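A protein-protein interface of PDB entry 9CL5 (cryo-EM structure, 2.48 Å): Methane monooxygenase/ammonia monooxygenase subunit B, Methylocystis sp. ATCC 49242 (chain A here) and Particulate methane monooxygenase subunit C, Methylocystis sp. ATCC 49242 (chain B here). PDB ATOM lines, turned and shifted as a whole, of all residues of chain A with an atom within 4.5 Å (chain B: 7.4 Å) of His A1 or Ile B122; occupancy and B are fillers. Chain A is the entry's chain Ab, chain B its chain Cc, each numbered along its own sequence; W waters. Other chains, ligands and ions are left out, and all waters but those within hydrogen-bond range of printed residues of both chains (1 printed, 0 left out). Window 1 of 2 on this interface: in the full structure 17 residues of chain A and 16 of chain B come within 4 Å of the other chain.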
ATOM      1  N   HIS A   1      -7.703  14.860  12.533  1.00  0.00           N
ATOM      2  CA  HIS A   1      -7.378  16.322  12.532  1.00  0.00           C
ATOM      3  C   HIS A   1      -6.848  16.810  13.889  1.00  0.00           C
ATOM      4  O   HIS A   1      -7.376  16.356  14.909  1.00  0.00           O
ATOM      5  CB  HIS A   1      -8.615  17.076  12.054  1.00  0.00           C
ATOM      6  CG  HIS A   1      -9.007  16.677  10.675  1.00  0.00           C
ATOM      7  ND1 HIS A   1      -8.756  15.433  10.129  1.00  0.00           N
ATOM      8  CD2 HIS A   1      -9.624  17.385   9.730  1.00  0.00           C
ATOM      9  CE1 HIS A   1      -9.215  15.419   8.889  1.00  0.00           C
ATOM     10  NE2 HIS A   1      -9.748  16.587   8.629  1.00  0.00           N
ATOM     11  N   GLY A   2      -5.848  17.703  13.910  1.00  0.00           N
ATOM     12  CA  GLY A   2      -5.282  18.263  15.157  1.00  0.00           C
ATOM     13  C   GLY A   2      -3.796  18.001  15.374  1.00  0.00           C
ATOM     14  O   GLY A   2      -3.188  18.768  16.131  1.00  0.00           O
ATOM     15  N   GLU A   3      -3.229  16.953  14.775  1.00  0.00           N
ATOM     16  CA  GLU A   3      -1.796  16.563  14.925  1.00  0.00           C
ATOM     17  C   GLU A   3      -0.836  17.653  14.403  1.00  0.00           C
ATOM     18  O   GLU A   3       0.133  17.930  15.098  1.00  0.00           O
ATOM     19  CB  GLU A   3      -1.599  15.207  14.244  1.00  0.00           C
ATOM     20  CG  GLU A   3      -2.028  15.158  12.780  1.00  0.00           C
ATOM     21  CD  GLU A   3      -3.498  14.921  12.481  1.00  0.00           C
ATOM     22  OE1 GLU A   3      -3.851  14.861  11.291  1.00  0.00           O
ATOM     23  OE2 GLU A   3      -4.297  14.813  13.425  1.00  0.00           O
ATOM     24  N   HIS A 105     -12.756  11.446   8.787  1.00  0.00           N
ATOM     25  CA  HIS A 105     -11.312  11.086   8.872  1.00  0.00           C
ATOM     26  C   HIS A 105     -11.085  10.347  10.185  1.00  0.00           C
ATOM     27  O   HIS A 105     -11.129  10.965  11.252  1.00  0.00           O
ATOM     28  CB  HIS A 105     -10.441  12.327   8.707  1.00  0.00           C
ATOM     29  CG  HIS A 105      -9.072  12.097   8.159  1.00  0.00           C
ATOM     30  ND1 HIS A 105      -7.906  12.386   8.842  1.00  0.00           N
ATOM     31  CD2 HIS A 105      -8.700  11.630   6.971  1.00  0.00           C
ATOM     32  CE1 HIS A 105      -6.879  12.087   8.069  1.00  0.00           C
ATOM     33  NE2 HIS A 105      -7.337  11.627   6.932  1.00  0.00           N
ATOM     34  N   HIS A 107      -8.755   8.088  12.683  1.00  0.00           N
ATOM     35  CA  HIS A 107      -7.324   7.861  12.942  1.00  0.00           C
ATOM     36  C   HIS A 107      -7.079   6.810  14.005  1.00  0.00           C
ATOM     37  O   HIS A 107      -8.004   6.454  14.753  1.00  0.00           O
ATOM     38  CB  HIS A 107      -6.742   9.125  13.574  1.00  0.00           C
ATOM     39  CG  HIS A 107      -6.629  10.323  12.702  1.00  0.00           C
ATOM     40  ND1 HIS A 107      -5.412  10.785  12.260  1.00  0.00           N
ATOM     41  CD2 HIS A 107      -7.541  11.163  12.225  1.00  0.00           C
ATOM     42  CE1 HIS A 107      -5.604  11.861  11.524  1.00  0.00           C
ATOM     43  NE2 HIS A 107      -6.888  12.107  11.491  1.00  0.00           N
ATOM     44  N   GLN A 109      -5.226   6.318  17.450  1.00  0.00           N
ATOM     45  CA  GLN A 109      -4.483   7.141  18.385  1.00  0.00           C
ATOM     46  C   GLN A 109      -4.295   6.394  19.696  1.00  0.00           C
ATOM     47  O   GLN A 109      -4.982   5.413  19.985  1.00  0.00           O
ATOM     48  CB  GLN A 109      -5.184   8.482  18.636  1.00  0.00           C
ATOM     49  CG  GLN A 109      -6.532   8.363  19.313  1.00  0.00           C
ATOM     50  CD  GLN A 109      -6.909   9.613  20.073  1.00  0.00           C
ATOM     51  OE1 GLN A 109      -6.062  10.255  20.692  1.00  0.00           O
ATOM     52  NE2 GLN A 109      -8.186   9.968  20.035  1.00  0.00           N
ATOM     53  N   ILE A 119      -1.482  10.967  17.970  1.00  0.00           N
ATOM     54  CA  ILE A 119      -2.387  10.678  16.864  1.00  0.00           C
ATOM     55  C   ILE A 119      -1.615  10.017  15.733  1.00  0.00           C
ATOM     56  O   ILE A 119      -0.539  10.485  15.340  1.00  0.00           O
ATOM     57  CB  ILE A 119      -3.087  11.963  16.381  1.00  0.00           C
ATOM     58  CG1 ILE A 119      -3.728  12.692  17.564  1.00  0.00           C
ATOM     59  CG2 ILE A 119      -4.120  11.645  15.319  1.00  0.00           C
ATOM     60  CD1 ILE A 119      -3.990  14.156  17.316  1.00  0.00           C
ATOM     61  N   TRP A 124     -10.120   8.633   5.171  1.00  0.00           N
ATOM     62  CA  TRP A 124     -11.497   9.054   4.947  1.00  0.00           C
ATOM     63  C   TRP A 124     -12.395   7.843   4.724  1.00  0.00           C
ATOM     64  O   TRP A 124     -12.150   7.031   3.827  1.00  0.00           O
ATOM     65  CB  TRP A 124     -11.578   9.994   3.744  1.00  0.00           C
ATOM     66  CG  TRP A 124     -10.912  11.312   3.963  1.00  0.00           C
ATOM     67  CD1 TRP A 124      -9.684  11.691   3.515  1.00  0.00           C
ATOM     68  CD2 TRP A 124     -11.439  12.428   4.687  1.00  0.00           C
ATOM     69  NE1 TRP A 124      -9.411  12.975   3.914  1.00  0.00           N
ATOM     70  CE2 TRP A 124     -10.473  13.450   4.635  1.00  0.00           C
ATOM     71  CE3 TRP A 124     -12.633  12.663   5.374  1.00  0.00           C
ATOM     72  CZ2 TRP A 124     -10.663  14.686   5.247  1.00  0.00           C
ATOM     73  CZ3 TRP A 124     -12.819  13.888   5.977  1.00  0.00           C
ATOM     74  CH2 TRP A 124     -11.842  14.884   5.910  1.00  0.00           C
ATOM     75  N   TRP B  32     -18.676  20.656  11.570  1.00  0.00           N
ATOM     76  CA  TRP B  32     -17.937  19.555  10.968  1.00  0.00           C
ATOM     77  C   TRP B  32     -17.329  19.922   9.621  1.00  0.00           C
ATOM     78  O   TRP B  32     -16.241  19.444   9.289  1.00  0.00           O
ATOM     79  CB  TRP B  32     -18.856  18.340  10.798  1.00  0.00           C
ATOM     80  CG  TRP B  32     -19.862  18.199  11.903  1.00  0.00           C
ATOM     81  CD1 TRP B  32     -21.131  18.703  11.923  1.00  0.00           C
ATOM     82  CD2 TRP B  32     -19.677  17.525  13.152  1.00  0.00           C
ATOM     83  NE1 TRP B  32     -21.749  18.378  13.107  1.00  0.00           N
ATOM     84  CE2 TRP B  32     -20.878  17.655  13.878  1.00  0.00           C
ATOM     85  CE3 TRP B  32     -18.615  16.824  13.728  1.00  0.00           C
ATOM     86  CZ2 TRP B  32     -21.043  17.108  15.148  1.00  0.00           C
ATOM     87  CZ3 TRP B  32     -18.783  16.283  14.988  1.00  0.00           C
ATOM     88  CH2 TRP B  32     -19.987  16.428  15.683  1.00  0.00           C
ATOM     89  N   GLY B  35     -14.980  23.383  11.051  1.00  0.00           N
ATOM     90  CA  GLY B  35     -14.450  23.569  12.389  1.00  0.00           C
ATOM     91  C   GLY B  35     -13.533  22.476  12.887  1.00  0.00           C
ATOM     92  O   GLY B  35     -12.948  22.623  13.964  1.00  0.00           O
ATOM     93  N   LEU B  36     -13.393  21.382  12.137  1.00  0.00           N
ATOM     94  CA  LEU B  36     -12.586  20.260  12.611  1.00  0.00           C
ATOM     95  C   LEU B  36     -11.093  20.553  12.498  1.00  0.00           C
ATOM     96  O   LEU B  36     -10.318  20.183  13.387  1.00  0.00           O
ATOM     97  CB  LEU B  36     -12.950  18.995  11.836  1.00  0.00           C
ATOM     98  CG  LEU B  36     -14.299  18.369  12.196  1.00  0.00           C
ATOM     99  CD1 LEU B  36     -14.432  16.986  11.583  1.00  0.00           C
ATOM    100  CD2 LEU B  36     -14.474  18.304  13.705  1.00  0.00           C
ATOM    101  N   ASP B  37     -10.671  21.210  11.421  1.00  0.00           N
ATOM    102  CA  ASP B  37      -9.261  21.484  11.167  1.00  0.00           C
ATOM    103  C   ASP B  37      -9.005  22.978  11.311  1.00  0.00           C
ATOM    104  O   ASP B  37      -9.670  23.790  10.659  1.00  0.00           O
ATOM    105  CB  ASP B  37      -8.849  21.001   9.777  1.00  0.00           C
ATOM    106  CG  ASP B  37      -7.349  20.851   9.634  1.00  0.00           C
ATOM    107  OD1 ASP B  37      -6.633  21.043  10.637  1.00  0.00           O
ATOM    108  OD2 ASP B  37      -6.886  20.539   8.516  1.00  0.00           O
ATOM    109  N   SER B  38      -8.039  23.334  12.160  1.00  0.00           N
ATOM    110  CA  SER B  38      -7.715  24.734  12.403  1.00  0.00           C
ATOM    111  C   SER B  38      -6.815  25.333  11.332  1.00  0.00           C
ATOM    112  O   SER B  38      -6.819  26.555  11.156  1.00  0.00           O
ATOM    113  CB  SER B  38      -7.048  24.886  13.770  1.00  0.00           C
ATOM    114  OG  SER B  38      -6.374  26.129  13.870  1.00  0.00           O
ATOM    115  N   ALA B  40      -7.005  24.538   8.073  1.00  0.00           N
ATOM    116  CA  ALA B  40      -7.675  24.521   6.784  1.00  0.00           C
ATOM    117  C   ALA B  40      -8.155  25.921   6.404  1.00  0.00           C
ATOM    118  O   ALA B  40      -8.484  26.730   7.276  1.00  0.00           O
ATOM    119  CB  ALA B  40      -8.858  23.560   6.816  1.00  0.00           C
ATOM    120  N   TRP B 117     -17.993  19.603  22.858  1.00  0.00           N
ATOM    121  CA  TRP B 117     -17.166  19.767  21.667  1.00  0.00           C
ATOM    122  C   TRP B 117     -15.729  19.331  21.925  1.00  0.00           C
ATOM    123  O   TRP B 117     -15.109  18.678  21.078  1.00  0.00           O
ATOM    124  CB  TRP B 117     -17.209  21.218  21.192  1.00  0.00           C
ATOM    125  CG  TRP B 117     -16.428  21.474  19.938  1.00  0.00           C
ATOM    126  CD1 TRP B 117     -15.218  22.095  19.840  1.00  0.00           C
ATOM    127  CD2 TRP B 117     -16.802  21.114  18.604  1.00  0.00           C
ATOM    128  NE1 TRP B 117     -14.817  22.147  18.529  1.00  0.00           N
ATOM    129  CE2 TRP B 117     -15.772  21.552  17.749  1.00  0.00           C
ATOM    130  CE3 TRP B 117     -17.909  20.464  18.047  1.00  0.00           C
ATOM    131  CZ2 TRP B 117     -15.815  21.361  16.371  1.00  0.00           C
ATOM    132  CZ3 TRP B 117     -17.950  20.277  16.680  1.00  0.00           C
ATOM    133  CH2 TRP B 117     -16.910  20.723  15.857  1.00  0.00           C
ATOM    134  N   HIS B 118     -15.183  19.676  23.093  1.00  0.00           N
ATOM    135  CA  HIS B 118     -13.821  19.267  23.415  1.00  0.00           C
ATOM    136  C   HIS B 118     -13.721  17.763  23.601  1.00  0.00           C
ATOM    137  O   HIS B 118     -12.658  17.180  23.362  1.00  0.00           O
ATOM    138  CB  HIS B 118     -13.332  19.987  24.669  1.00  0.00           C
ATOM    139  CG  HIS B 118     -13.023  21.433  24.449  1.00  0.00           C
ATOM    140  ND1 HIS B 118     -12.352  21.889  23.333  1.00  0.00           N
ATOM    141  CD2 HIS B 118     -13.282  22.525  25.204  1.00  0.00           C
ATOM    142  CE1 HIS B 118     -12.222  23.201  23.409  1.00  0.00           C
ATOM    143  NE2 HIS B 118     -12.776  23.613  24.534  1.00  0.00           N
ATOM    144  N   MET B 119     -14.805  17.120  24.030  1.00  0.00           N
ATOM    145  CA  MET B 119     -14.785  15.670  24.138  1.00  0.00           C
ATOM    146  C   MET B 119     -14.926  14.978  22.789  1.00  0.00           C
ATOM    147  O   MET B 119     -14.523  13.816  22.666  1.00  0.00           O
ATOM    148  CB  MET B 119     -15.889  15.193  25.079  1.00  0.00           C
ATOM    149  CG  MET B 119     -15.360  14.454  26.291  1.00  0.00           C
ATOM    150  SD  MET B 119     -14.157  15.422  27.219  1.00  0.00           S
ATOM    151  CE  MET B 119     -15.234  16.332  28.323  1.00  0.00           C
ATOM    152  N   THR B 120     -15.486  15.645  21.781  1.00  0.00           N
ATOM    153  CA  THR B 120     -15.579  15.008  20.469  1.00  0.00           C
ATOM    154  C   THR B 120     -14.375  15.259  19.571  1.00  0.00           C
ATOM    155  O   THR B 120     -14.093  14.433  18.695  1.00  0.00           O
ATOM    156  CB  THR B 120     -16.836  15.466  19.730  1.00  0.00           C
ATOM    157  OG1 THR B 120     -16.715  16.850  19.378  1.00  0.00           O
ATOM    158  CG2 THR B 120     -18.037  15.262  20.599  1.00  0.00           C
ATOM    159  N   VAL B 121     -13.656  16.365  19.748  1.00  0.00           N
ATOM    160  CA  VAL B 121     -12.559  16.705  18.853  1.00  0.00           C
ATOM    161  C   VAL B 121     -11.254  16.724  19.634  1.00  0.00           C
ATOM    162  O   VAL B 121     -11.229  16.796  20.864  1.00  0.00           O
ATOM    163  CB  VAL B 121     -12.776  18.056  18.140  1.00  0.00           C
ATOM    164  CG1 VAL B 121     -14.130  18.087  17.450  1.00  0.00           C
ATOM    165  CG2 VAL B 121     -12.633  19.209  19.121  1.00  0.00           C
ATOM    166  N   ILE B 122     -10.155  16.652  18.890  1.00  0.00           N
ATOM    167  CA  ILE B 122      -8.820  16.830  19.444  1.00  0.00           C
ATOM    168  C   ILE B 122      -8.455  18.300  19.294  1.00  0.00           C
ATOM    169  O   ILE B 122      -8.429  18.829  18.176  1.00  0.00           O
ATOM    170  CB  ILE B 122      -7.795  15.929  18.736  1.00  0.00           C
ATOM    171  CG1 ILE B 122      -7.948  14.478  19.196  1.00  0.00           C
ATOM    172  CG2 ILE B 122      -6.381  16.424  18.992  1.00  0.00           C
ATOM    173  CD1 ILE B 122      -7.784  14.291  20.685  1.00  0.00           C
ATOM    174  N   ARG B 123      -8.183  18.963  20.413  1.00  0.00           N
ATOM    175  CA  ARG B 123      -7.939  20.397  20.386  1.00  0.00           C
ATOM    176  C   ARG B 123      -6.643  20.701  19.646  1.00  0.00           C
ATOM    177  O   ARG B 123      -5.608  20.079  19.899  1.00  0.00           O
ATOM    178  CB  ARG B 123      -7.890  20.954  21.807  1.00  0.00           C
ATOM    179  CG  ARG B 123      -8.657  22.252  21.969  1.00  0.00           C
ATOM    180  CD  ARG B 123      -8.812  22.638  23.428  1.00  0.00           C
ATOM    181  NE  ARG B 123      -7.904  23.709  23.815  1.00  0.00           N
ATOM    182  CZ  ARG B 123      -7.896  24.280  25.013  1.00  0.00           C
ATOM    183  NH1 ARG B 123      -8.741  23.911  25.960  1.00  0.00           N
ATOM    184  NH2 ARG B 123      -7.019  25.249  25.262  1.00  0.00           N
ATOM    185  N   ASP B 124      -6.708  21.658  18.719  1.00  0.00           N
ATOM    186  CA  ASP B 124      -5.564  22.036  17.910  1.00  0.00           C
ATOM    187  C   ASP B 124      -5.278  23.528  17.916  1.00  0.00           C
ATOM    188  O   ASP B 124      -4.295  23.951  17.296  1.00  0.00           O
ATOM    189  CB  ASP B 124      -5.759  21.574  16.457  1.00  0.00           C
ATOM    190  CG  ASP B 124      -7.113  21.957  15.901  1.00  0.00           C
ATOM    191  OD1 ASP B 124      -7.919  22.550  16.646  1.00  0.00           O
ATOM    192  OD2 ASP B 124      -7.369  21.667  14.714  1.00  0.00           O
ATOM    193  N   THR B 125      -6.097  24.334  18.584  1.00  0.00           N
ATOM    194  CA  THR B 125      -5.898  25.775  18.597  1.00  0.00           C
ATOM    195  C   THR B 125      -6.607  26.358  19.809  1.00  0.00           C
ATOM    196  O   THR B 125      -7.460  25.713  20.425  1.00  0.00           O
ATOM    197  CB  THR B 125      -6.412  26.426  17.308  1.00  0.00           C
ATOM    198  OG1 THR B 125      -6.120  27.829  17.325  1.00  0.00           O
ATOM    199  CG2 THR B 125      -7.908  26.218  17.164  1.00  0.00           C
ATOM    200  N   THR B 128     -11.221  27.483  19.032  1.00  0.00           N
ATOM    201  CA  THR B 128     -12.112  26.489  18.456  1.00  0.00           C
ATOM    202  C   THR B 128     -13.486  27.103  18.237  1.00  0.00           C
ATOM    203  O   THR B 128     -13.814  28.131  18.838  1.00  0.00           O
ATOM    204  CB  THR B 128     -12.212  25.272  19.377  1.00  0.00           C
ATOM    205  OG1 THR B 128     -12.676  25.680  20.669  1.00  0.00           O
ATOM    206  CG2 THR B 128     -10.855  24.604  19.524  1.00  0.00           C
ATOM    207  N   GLU B 196      -8.594  16.453  29.134  1.00  0.00           N
ATOM    208  CA  GLU B 196      -9.825  17.242  29.053  1.00  0.00           C
ATOM    209  C   GLU B 196     -10.789  16.820  30.162  1.00  0.00           C
ATOM    210  O   GLU B 196     -11.796  16.146  29.944  1.00  0.00           O
ATOM    211  CB  GLU B 196     -10.458  17.099  27.674  1.00  0.00           C
ATOM    212  CG  GLU B 196      -9.533  17.455  26.528  1.00  0.00           C
ATOM    213  CD  GLU B 196      -9.780  18.852  26.001  1.00  0.00           C
ATOM    214  OE1 GLU B 196     -10.272  19.700  26.773  1.00  0.00           O
ATOM    215  OE2 GLU B 196      -9.483  19.103  24.817  1.00  0.00           O
HETATM  216  O   HOH W   1      -9.906  16.884  15.867  1.00  0.00           O
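The backbone NH (N) of Ser B38 is in hydrogen-bond range of the side-chain carboxylate (OD2) of Asp B124, 3.1 Å away.
His A1 touches Leu B36 (CB to O, 3.8 Å). CB of Asp B37 touches CD2 of His A1, 3.7 Å away. O of His A1 touches CB of Ile B122, at 3.9 Å. Asp B124 touches Gly A2 (CB to CA, 3.6 Å). Ile A119 touches Ile B122.
Of the printed residues of chain B, Ile A119 touches Ile B122. Of the printed residues of chain A, Asp B37 touches His A1. Ile B122 touches just these residues of chain A: His A1 and Ile A119.
Of the 8 printed residues of chain A, 3 touch a printed residue of chain B. Hydrophobic or aromatic side chains of chain A within 4 Å of the printed part of chain B: His A1 and Ile A119. Hydrophobic or aromatic side chains of chain B within 4 Å of the printed part of chain A: Ile B122. Among the printed residues, 5 pairs touch across the chains.
Water W1 lies within hydrogen-bond range of O of His A1 (2.8 Å) and N of Ile B122 (3.0 Å).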
